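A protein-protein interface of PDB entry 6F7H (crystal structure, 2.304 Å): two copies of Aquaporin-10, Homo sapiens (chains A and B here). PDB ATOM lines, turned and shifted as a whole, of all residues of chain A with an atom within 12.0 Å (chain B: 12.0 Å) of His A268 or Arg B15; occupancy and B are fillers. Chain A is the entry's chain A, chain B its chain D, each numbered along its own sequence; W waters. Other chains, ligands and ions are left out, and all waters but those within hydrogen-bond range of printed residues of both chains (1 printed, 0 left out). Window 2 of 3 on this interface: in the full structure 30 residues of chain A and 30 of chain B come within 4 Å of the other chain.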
ATOM      1  N   ASP A 179       4.342  17.524   5.120  1.00  0.00           N
ATOM      2  CA  ASP A 179       4.365  18.736   4.331  1.00  0.00           C
ATOM      3  C   ASP A 179       5.250  19.796   4.937  1.00  0.00           C
ATOM      4  O   ASP A 179       4.902  20.414   5.912  1.00  0.00           O
ATOM      5  CB  ASP A 179       2.948  19.268   4.171  1.00  0.00           C
ATOM      6  CG  ASP A 179       2.813  20.227   3.037  1.00  0.00           C
ATOM      7  OD1 ASP A 179       3.831  20.712   2.567  1.00  0.00           O
ATOM      8  OD2 ASP A 179       1.698  20.491   2.612  1.00  0.00           O
ATOM      9  N   ARG A 181       5.902  22.751   4.078  1.00  0.00           N
ATOM     10  CA  ARG A 181       5.464  24.135   4.097  1.00  0.00           C
ATOM     11  C   ARG A 181       4.541  24.486   5.244  1.00  0.00           C
ATOM     12  O   ARG A 181       4.161  25.611   5.427  1.00  0.00           O
ATOM     13  CB  ARG A 181       4.983  24.625   2.739  1.00  0.00           C
ATOM     14  CG  ARG A 181       3.826  23.884   2.157  1.00  0.00           C
ATOM     15  CD  ARG A 181       4.065  23.569   0.706  1.00  0.00           C
ATOM     16  NE  ARG A 181       3.290  22.406   0.369  1.00  0.00           N
ATOM     17  CZ  ARG A 181       2.442  22.333  -0.632  1.00  0.00           C
ATOM     18  NH1 ARG A 181       2.293  23.360  -1.435  1.00  0.00           N
ATOM     19  NH2 ARG A 181       1.767  21.225  -0.838  1.00  0.00           N
ATOM     20  N   ASN A 182       4.206  23.466   6.003  1.00  0.00           N
ATOM     21  CA  ASN A 182       3.341  23.615   7.139  1.00  0.00           C
ATOM     22  C   ASN A 182       4.196  23.861   8.331  1.00  0.00           C
ATOM     23  O   ASN A 182       5.216  23.249   8.484  1.00  0.00           O
ATOM     24  CB  ASN A 182       2.573  22.333   7.402  1.00  0.00           C
ATOM     25  CG  ASN A 182       1.418  22.138   6.470  1.00  0.00           C
ATOM     26  OD1 ASN A 182       1.127  21.038   6.066  1.00  0.00           O
ATOM     27  ND2 ASN A 182       0.763  23.203   6.125  1.00  0.00           N
ATOM     28  N   THR A 259      -8.827  14.804   0.638  1.00  0.00           N
ATOM     29  CA  THR A 259      -9.156  15.871   1.573  1.00  0.00           C
ATOM     30  C   THR A 259      -7.962  16.785   1.791  1.00  0.00           C
ATOM     31  O   THR A 259      -8.098  18.018   1.781  1.00  0.00           O
ATOM     32  CB  THR A 259      -9.605  15.292   2.906  1.00  0.00           C
ATOM     33  OG1 THR A 259     -10.720  14.426   2.697  1.00  0.00           O
ATOM     34  CG2 THR A 259     -10.002  16.411   3.855  1.00  0.00           C
ATOM     35  N   TYR A 260      -6.777  16.195   1.989  1.00  0.00           N
ATOM     36  CA  TYR A 260      -5.597  17.005   2.269  1.00  0.00           C
ATOM     37  C   TYR A 260      -5.199  17.831   1.048  1.00  0.00           C
ATOM     38  O   TYR A 260      -4.912  19.027   1.167  1.00  0.00           O
ATOM     39  CB  TYR A 260      -4.401  16.149   2.745  1.00  0.00           C
ATOM     40  CG  TYR A 260      -3.245  17.067   3.081  1.00  0.00           C
ATOM     41  CD1 TYR A 260      -3.244  17.793   4.264  1.00  0.00           C
ATOM     42  CD2 TYR A 260      -2.189  17.252   2.201  1.00  0.00           C
ATOM     43  CE1 TYR A 260      -2.215  18.671   4.576  1.00  0.00           C
ATOM     44  CE2 TYR A 260      -1.133  18.116   2.510  1.00  0.00           C
ATOM     45  CZ  TYR A 260      -1.166  18.833   3.694  1.00  0.00           C
ATOM     46  OH  TYR A 260      -0.149  19.696   4.021  1.00  0.00           O
ATOM     47  N   GLN A 261      -5.139  17.199  -0.127  1.00  0.00           N
ATOM     48  CA  GLN A 261      -4.884  17.940  -1.362  1.00  0.00           C
ATOM     49  C   GLN A 261      -5.889  19.075  -1.554  1.00  0.00           C
ATOM     50  O   GLN A 261      -5.512  20.176  -1.964  1.00  0.00           O
ATOM     51  CB  GLN A 261      -4.923  16.997  -2.555  1.00  0.00           C
ATOM     52  CG  GLN A 261      -3.904  15.885  -2.463  1.00  0.00           C
ATOM     53  CD  GLN A 261      -2.500  16.405  -2.657  1.00  0.00           C
ATOM     54  OE1 GLN A 261      -1.951  17.093  -1.788  1.00  0.00           O
ATOM     55  NE2 GLN A 261      -1.920  16.119  -3.825  1.00  0.00           N
ATOM     56  N   LEU A 262      -7.168  18.836  -1.264  1.00  0.00           N
ATOM     57  CA  LEU A 262      -8.142  19.914  -1.417  1.00  0.00           C
ATOM     58  C   LEU A 262      -7.822  21.056  -0.453  1.00  0.00           C
ATOM     59  O   LEU A 262      -7.755  22.232  -0.859  1.00  0.00           O
ATOM     60  CB  LEU A 262      -9.579  19.393  -1.222  1.00  0.00           C
ATOM     61  CG  LEU A 262     -10.743  20.410  -1.122  1.00  0.00           C
ATOM     62  CD1 LEU A 262     -10.961  21.235  -2.391  1.00  0.00           C
ATOM     63  CD2 LEU A 262     -12.045  19.736  -0.768  1.00  0.00           C
ATOM     64  N   LEU A 263      -7.598  20.723   0.829  1.00  0.00           N
ATOM     65  CA  LEU A 263      -7.279  21.754   1.817  1.00  0.00           C
ATOM     66  C   LEU A 263      -6.074  22.580   1.378  1.00  0.00           C
ATOM     67  O   LEU A 263      -6.066  23.806   1.514  1.00  0.00           O
ATOM     68  CB  LEU A 263      -7.009  21.120   3.181  1.00  0.00           C
ATOM     69  CG  LEU A 263      -8.274  20.561   3.818  1.00  0.00           C
ATOM     70  CD1 LEU A 263      -7.876  19.718   5.029  1.00  0.00           C
ATOM     71  CD2 LEU A 263      -9.163  21.697   4.212  1.00  0.00           C
ATOM     72  N   VAL A 264      -5.043  21.924   0.855  1.00  0.00           N
ATOM     73  CA  VAL A 264      -3.914  22.674   0.338  1.00  0.00           C
ATOM     74  C   VAL A 264      -4.366  23.584  -0.794  1.00  0.00           C
ATOM     75  O   VAL A 264      -3.954  24.746  -0.870  1.00  0.00           O
ATOM     76  CB  VAL A 264      -2.788  21.730  -0.114  1.00  0.00           C
ATOM     77  CG1 VAL A 264      -1.768  22.535  -0.882  1.00  0.00           C
ATOM     78  CG2 VAL A 264      -2.123  21.043   1.125  1.00  0.00           C
ATOM     79  N   ALA A 265      -5.216  23.072  -1.699  1.00  0.00           N
ATOM     80  CA  ALA A 265      -5.614  23.901  -2.839  1.00  0.00           C
ATOM     81  C   ALA A 265      -6.441  25.099  -2.367  1.00  0.00           C
ATOM     82  O   ALA A 265      -6.348  26.186  -2.940  1.00  0.00           O
ATOM     83  CB  ALA A 265      -6.374  23.062  -3.869  1.00  0.00           C
ATOM     84  N   LEU A 266      -7.213  24.934  -1.324  1.00  0.00           N
ATOM     85  CA  LEU A 266      -7.995  26.036  -0.861  1.00  0.00           C
ATOM     86  C   LEU A 266      -7.143  27.076  -0.200  1.00  0.00           C
ATOM     87  O   LEU A 266      -7.561  28.191  -0.032  1.00  0.00           O
ATOM     88  CB  LEU A 266      -9.037  25.560   0.132  1.00  0.00           C
ATOM     89  CG  LEU A 266     -10.205  24.738  -0.374  1.00  0.00           C
ATOM     90  CD1 LEU A 266     -11.028  24.202   0.763  1.00  0.00           C
ATOM     91  CD2 LEU A 266     -11.074  25.530  -1.312  1.00  0.00           C
ATOM     92  N   HIS A 267      -5.938  26.702   0.191  1.00  0.00           N
ATOM     93  CA  HIS A 267      -5.086  27.626   0.904  1.00  0.00           C
ATOM     94  C   HIS A 267      -3.973  28.274   0.120  1.00  0.00           C
ATOM     95  O   HIS A 267      -3.454  29.270   0.536  1.00  0.00           O
ATOM     96  CB  HIS A 267      -4.586  26.997   2.194  1.00  0.00           C
ATOM     97  CG  HIS A 267      -5.642  26.863   3.241  1.00  0.00           C
ATOM     98  ND1 HIS A 267      -6.466  25.770   3.330  1.00  0.00           N
ATOM     99  CD2 HIS A 267      -6.000  27.682   4.249  1.00  0.00           C
ATOM    100  CE1 HIS A 267      -7.288  25.923   4.344  1.00  0.00           C
ATOM    101  NE2 HIS A 267      -7.024  27.073   4.921  1.00  0.00           N
ATOM    102  N   HIS A 268      -3.632  27.716  -1.024  1.00  0.00           N
ATOM    103  CA  HIS A 268      -2.623  28.269  -1.914  1.00  0.00           C
ATOM    104  C   HIS A 268      -2.172  27.276  -2.955  1.00  0.00           C
ATOM    105  O   HIS A 268      -2.780  27.178  -4.006  1.00  0.00           O
ATOM    106  CB  HIS A 268      -1.421  28.818  -1.177  1.00  0.00           C
ATOM    107  CG  HIS A 268      -1.025  30.180  -1.637  1.00  0.00           C
ATOM    108  ND1 HIS A 268      -0.532  31.141  -0.786  1.00  0.00           N
ATOM    109  CD2 HIS A 268      -1.072  30.751  -2.861  1.00  0.00           C
ATOM    110  CE1 HIS A 268      -0.288  32.244  -1.466  1.00  0.00           C
ATOM    111  NE2 HIS A 268      -0.608  32.035  -2.728  1.00  0.00           N
ATOM    112  N   HIS B  13      -6.712  27.712  -8.710  1.00  0.00           N
ATOM    113  CA  HIS B  13      -8.010  28.312  -9.020  1.00  0.00           C
ATOM    114  C   HIS B  13      -9.051  28.081  -7.921  1.00  0.00           C
ATOM    115  O   HIS B  13     -10.125  28.689  -7.942  1.00  0.00           O
ATOM    116  CB  HIS B  13      -8.537  27.787 -10.354  1.00  0.00           C
ATOM    117  CG  HIS B  13      -7.900  28.429 -11.542  1.00  0.00           C
ATOM    118  ND1 HIS B  13      -7.760  29.796 -11.667  1.00  0.00           N
ATOM    119  CD2 HIS B  13      -7.345  27.890 -12.654  1.00  0.00           C
ATOM    120  CE1 HIS B  13      -7.166  30.072 -12.819  1.00  0.00           C
ATOM    121  NE2 HIS B  13      -6.900  28.933 -13.435  1.00  0.00           N
ATOM    122  N   LEU B  14      -8.730  27.224  -6.960  1.00  0.00           N
ATOM    123  CA  LEU B  14      -9.579  26.989  -5.797  1.00  0.00           C
ATOM    124  C   LEU B  14      -9.224  27.849  -4.600  1.00  0.00           C
ATOM    125  O   LEU B  14      -9.845  27.672  -3.553  1.00  0.00           O
ATOM    126  CB  LEU B  14      -9.520  25.523  -5.350  1.00  0.00           C
ATOM    127  CG  LEU B  14     -10.260  24.530  -6.243  1.00  0.00           C
ATOM    128  CD1 LEU B  14     -10.279  23.147  -5.615  1.00  0.00           C
ATOM    129  CD2 LEU B  14     -11.703  25.031  -6.587  1.00  0.00           C
ATOM    130  N   ARG B  15      -8.245  28.752  -4.702  1.00  0.00           N
ATOM    131  CA  ARG B  15      -7.778  29.471  -3.514  1.00  0.00           C
ATOM    132  C   ARG B  15      -8.878  30.359  -2.939  1.00  0.00           C
ATOM    133  O   ARG B  15      -9.487  31.153  -3.655  1.00  0.00           O
ATOM    134  CB  ARG B  15      -6.544  30.323  -3.839  1.00  0.00           C
ATOM    135  CG  ARG B  15      -5.749  30.731  -2.593  1.00  0.00           C
ATOM    136  CD  ARG B  15      -4.570  31.631  -2.944  1.00  0.00           C
ATOM    137  NE  ARG B  15      -5.021  32.780  -3.724  1.00  0.00           N
ATOM    138  CZ  ARG B  15      -5.329  33.964  -3.202  1.00  0.00           C
ATOM    139  NH1 ARG B  15      -5.220  34.155  -1.888  1.00  0.00           N
ATOM    140  NH2 ARG B  15      -5.745  34.949  -3.998  1.00  0.00           N
ATOM    141  N   ILE B  16      -9.115  30.235  -1.638  1.00  0.00           N
ATOM    142  CA  ILE B  16     -10.030  31.117  -0.920  1.00  0.00           C
ATOM    143  C   ILE B  16      -9.312  32.445  -0.695  1.00  0.00           C
ATOM    144  O   ILE B  16      -8.298  32.495   0.002  1.00  0.00           O
ATOM    145  CB  ILE B  16     -10.459  30.498   0.417  1.00  0.00           C
ATOM    146  CG1 ILE B  16     -11.184  29.154   0.232  1.00  0.00           C
ATOM    147  CG2 ILE B  16     -11.219  31.523   1.298  1.00  0.00           C
ATOM    148  CD1 ILE B  16     -11.172  28.332   1.545  1.00  0.00           C
ATOM    149  N   ARG B  17      -9.836  33.533  -1.265  1.00  0.00           N
ATOM    150  CA  ARG B  17      -9.150  34.819  -1.101  1.00  0.00           C
ATOM    151  C   ARG B  17      -9.614  35.548   0.149  1.00  0.00           C
ATOM    152  O   ARG B  17      -8.838  36.267   0.782  1.00  0.00           O
ATOM    153  CB  ARG B  17      -9.354  35.699  -2.322  1.00  0.00           C
ATOM    154  CG  ARG B  17      -8.528  35.292  -3.500  1.00  0.00           C
ATOM    155  CD  ARG B  17      -9.282  35.623  -4.763  1.00  0.00           C
ATOM    156  NE  ARG B  17     -10.657  35.157  -4.628  1.00  0.00           N
ATOM    157  CZ  ARG B  17     -11.558  35.154  -5.602  1.00  0.00           C
ATOM    158  NH1 ARG B  17     -11.235  35.591  -6.810  1.00  0.00           N
ATOM    159  NH2 ARG B  17     -12.783  34.711  -5.358  1.00  0.00           N
ATOM    160  N   SER B  18     -10.865  35.363   0.525  1.00  0.00           N
ATOM    161  CA  SER B  18     -11.401  35.987   1.722  1.00  0.00           C
ATOM    162  C   SER B  18     -10.738  35.441   2.986  1.00  0.00           C
ATOM    163  O   SER B  18     -10.697  34.223   3.208  1.00  0.00           O
ATOM    164  CB  SER B  18     -12.906  35.744   1.762  1.00  0.00           C
ATOM    165  OG  SER B  18     -13.402  35.759   3.075  1.00  0.00           O
ATOM    166  N   LEU B  19     -10.241  36.350   3.829  1.00  0.00           N
ATOM    167  CA  LEU B  19      -9.624  35.944   5.101  1.00  0.00           C
ATOM    168  C   LEU B  19     -10.654  35.353   6.059  1.00  0.00           C
ATOM    169  O   LEU B  19     -10.392  34.346   6.730  1.00  0.00           O
ATOM    170  CB  LEU B  19      -8.918  37.142   5.740  1.00  0.00           C
ATOM    171  CG  LEU B  19      -8.317  37.012   7.137  1.00  0.00           C
ATOM    172  CD1 LEU B  19      -7.303  35.868   7.211  1.00  0.00           C
ATOM    173  CD2 LEU B  19      -7.682  38.346   7.559  1.00  0.00           C
ATOM    174  N   LEU B  20     -11.835  35.960   6.126  1.00  0.00           N
ATOM    175  CA  LEU B  20     -12.877  35.453   7.006  1.00  0.00           C
ATOM    176  C   LEU B  20     -13.228  34.006   6.666  1.00  0.00           C
ATOM    177  O   LEU B  20     -13.331  33.155   7.563  1.00  0.00           O
ATOM    178  CB  LEU B  20     -14.099  36.369   6.916  1.00  0.00           C
ATOM    179  CG  LEU B  20     -15.251  36.017   7.849  1.00  0.00           C
ATOM    180  CD1 LEU B  20     -14.760  35.746   9.280  1.00  0.00           C
ATOM    181  CD2 LEU B  20     -16.238  37.142   7.850  1.00  0.00           C
ATOM    182  N   ALA B  21     -13.392  33.703   5.376  1.00  0.00           N
ATOM    183  CA  ALA B  21     -13.697  32.333   4.964  1.00  0.00           C
ATOM    184  C   ALA B  21     -12.611  31.358   5.437  1.00  0.00           C
ATOM    185  O   ALA B  21     -12.910  30.296   5.993  1.00  0.00           O
ATOM    186  CB  ALA B  21     -13.875  32.284   3.442  1.00  0.00           C
ATOM    187  N   ARG B  22     -11.341  31.713   5.231  1.00  0.00           N
ATOM    188  CA  ARG B  22     -10.243  30.884   5.730  1.00  0.00           C
ATOM    189  C   ARG B  22     -10.324  30.690   7.244  1.00  0.00           C
ATOM    190  O   ARG B  22     -10.136  29.571   7.738  1.00  0.00           O
ATOM    191  CB  ARG B  22      -8.891  31.485   5.327  1.00  0.00           C
ATOM    192  CG  ARG B  22      -8.584  31.282   3.826  1.00  0.00           C
ATOM    193  CD  ARG B  22      -7.180  31.707   3.447  1.00  0.00           C
ATOM    194  NE  ARG B  22      -6.865  33.060   3.893  1.00  0.00           N
ATOM    195  CZ  ARG B  22      -6.843  34.127   3.093  1.00  0.00           C
ATOM    196  NH1 ARG B  22      -7.135  34.003   1.798  1.00  0.00           N
ATOM    197  NH2 ARG B  22      -6.532  35.322   3.587  1.00  0.00           N
ATOM    198  N   GLN B  23     -10.605  31.759   7.995  1.00  0.00           N
ATOM    199  CA  GLN B  23     -10.711  31.632   9.449  1.00  0.00           C
ATOM    200  C   GLN B  23     -11.833  30.685   9.831  1.00  0.00           C
ATOM    201  O   GLN B  23     -11.655  29.826  10.705  1.00  0.00           O
ATOM    202  CB  GLN B  23     -10.921  33.003  10.086  1.00  0.00           C
ATOM    203  CG  GLN B  23      -9.674  33.870  10.059  1.00  0.00           C
ATOM    204  CD  GLN B  23      -9.995  35.341  10.221  1.00  0.00           C
ATOM    205  OE1 GLN B  23     -11.130  35.761  10.035  1.00  0.00           O
ATOM    206  NE2 GLN B  23      -8.997  36.129  10.563  1.00  0.00           N
ATOM    207  N   LEU B  25     -13.138  28.229   8.045  1.00  0.00           N
ATOM    208  CA  LEU B  25     -12.762  26.855   7.740  1.00  0.00           C
ATOM    209  C   LEU B  25     -11.884  26.255   8.850  1.00  0.00           C
ATOM    210  O   LEU B  25     -12.062  25.086   9.236  1.00  0.00           O
ATOM    211  CB  LEU B  25     -12.052  26.818   6.382  1.00  0.00           C
ATOM    212  CG  LEU B  25     -11.617  25.441   5.879  1.00  0.00           C
ATOM    213  CD1 LEU B  25     -12.837  24.521   5.882  1.00  0.00           C
ATOM    214  CD2 LEU B  25     -11.036  25.534   4.479  1.00  0.00           C
HETATM  215  O   HOH W   1      -8.314  27.767   7.176  1.00  0.00           O
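Of the printed residues of chain B, Leu A262 touches Leu B14 (3.8 Å).
Ala A265 touches two residues of chain B.
Of chain B, only Leu B25 (3.8 Å) comes within 4 Å of His A267.
Of chain B, only Arg B15 comes within 4 Å of His A268.
Of chain A, only Ala A265 (3.6 Å), Leu A266 (3.7 Å) and His A268 (3.6 Å) come within 4 Å of Arg B15.
Ile B16 touches just one residue of chain A: Leu A266 (3.0 Å).
Of the printed residues of chain A, Leu B25 touches Leu A266 and His A267.
The nearest residue of chain B that does not touch His A268 is Ile B16 (6.1 Å).
The nearest printed residue of chain A that does not touch Leu B25 is Leu A263 (4.3 Å).
No position is printed for both chains.
Water W1 lies within hydrogen-bond range of O of Arg B22 (2.6 Å) and NE2 of His A267 (2.7 Å).
N of Ile B16 sits at hydrogen-bond distance from O of Leu A266 (3.0 Å).
Of the 13 printed residues of chain A, 5 touch a printed residue of chain B.
Printed residues of chain A that touch a printed residue of chain B: Leu A262, Ala A265, Leu A266, His A267 and His A268.
Hydrophobic or aromatic side chains of chain A that line the printed part of chain B: Leu A262, Leu A266, His A267 and His A268.
Among the printed residues, 9 pairs touch across the chains.
Among the printed residues, pairs that only touch across the chains: Leu A266 with Leu B14, His A268 with Arg B15, Ala A265 with Arg B15, Ala A265 with Leu B14, Leu A266 with Arg B15, His A267 with Leu B25, Leu A262 with Leu B14 and Leu A266 with Leu B25.
ND1 of His A267 is in hydrogen-bond range of O of Leu A263 (2.7 Å).
The backbone carbonyl oxygen (O) of Ile B16 lies within hydrogen-bond range of the guanidinium group (NH1) of Arg B22 (2.6 Å).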
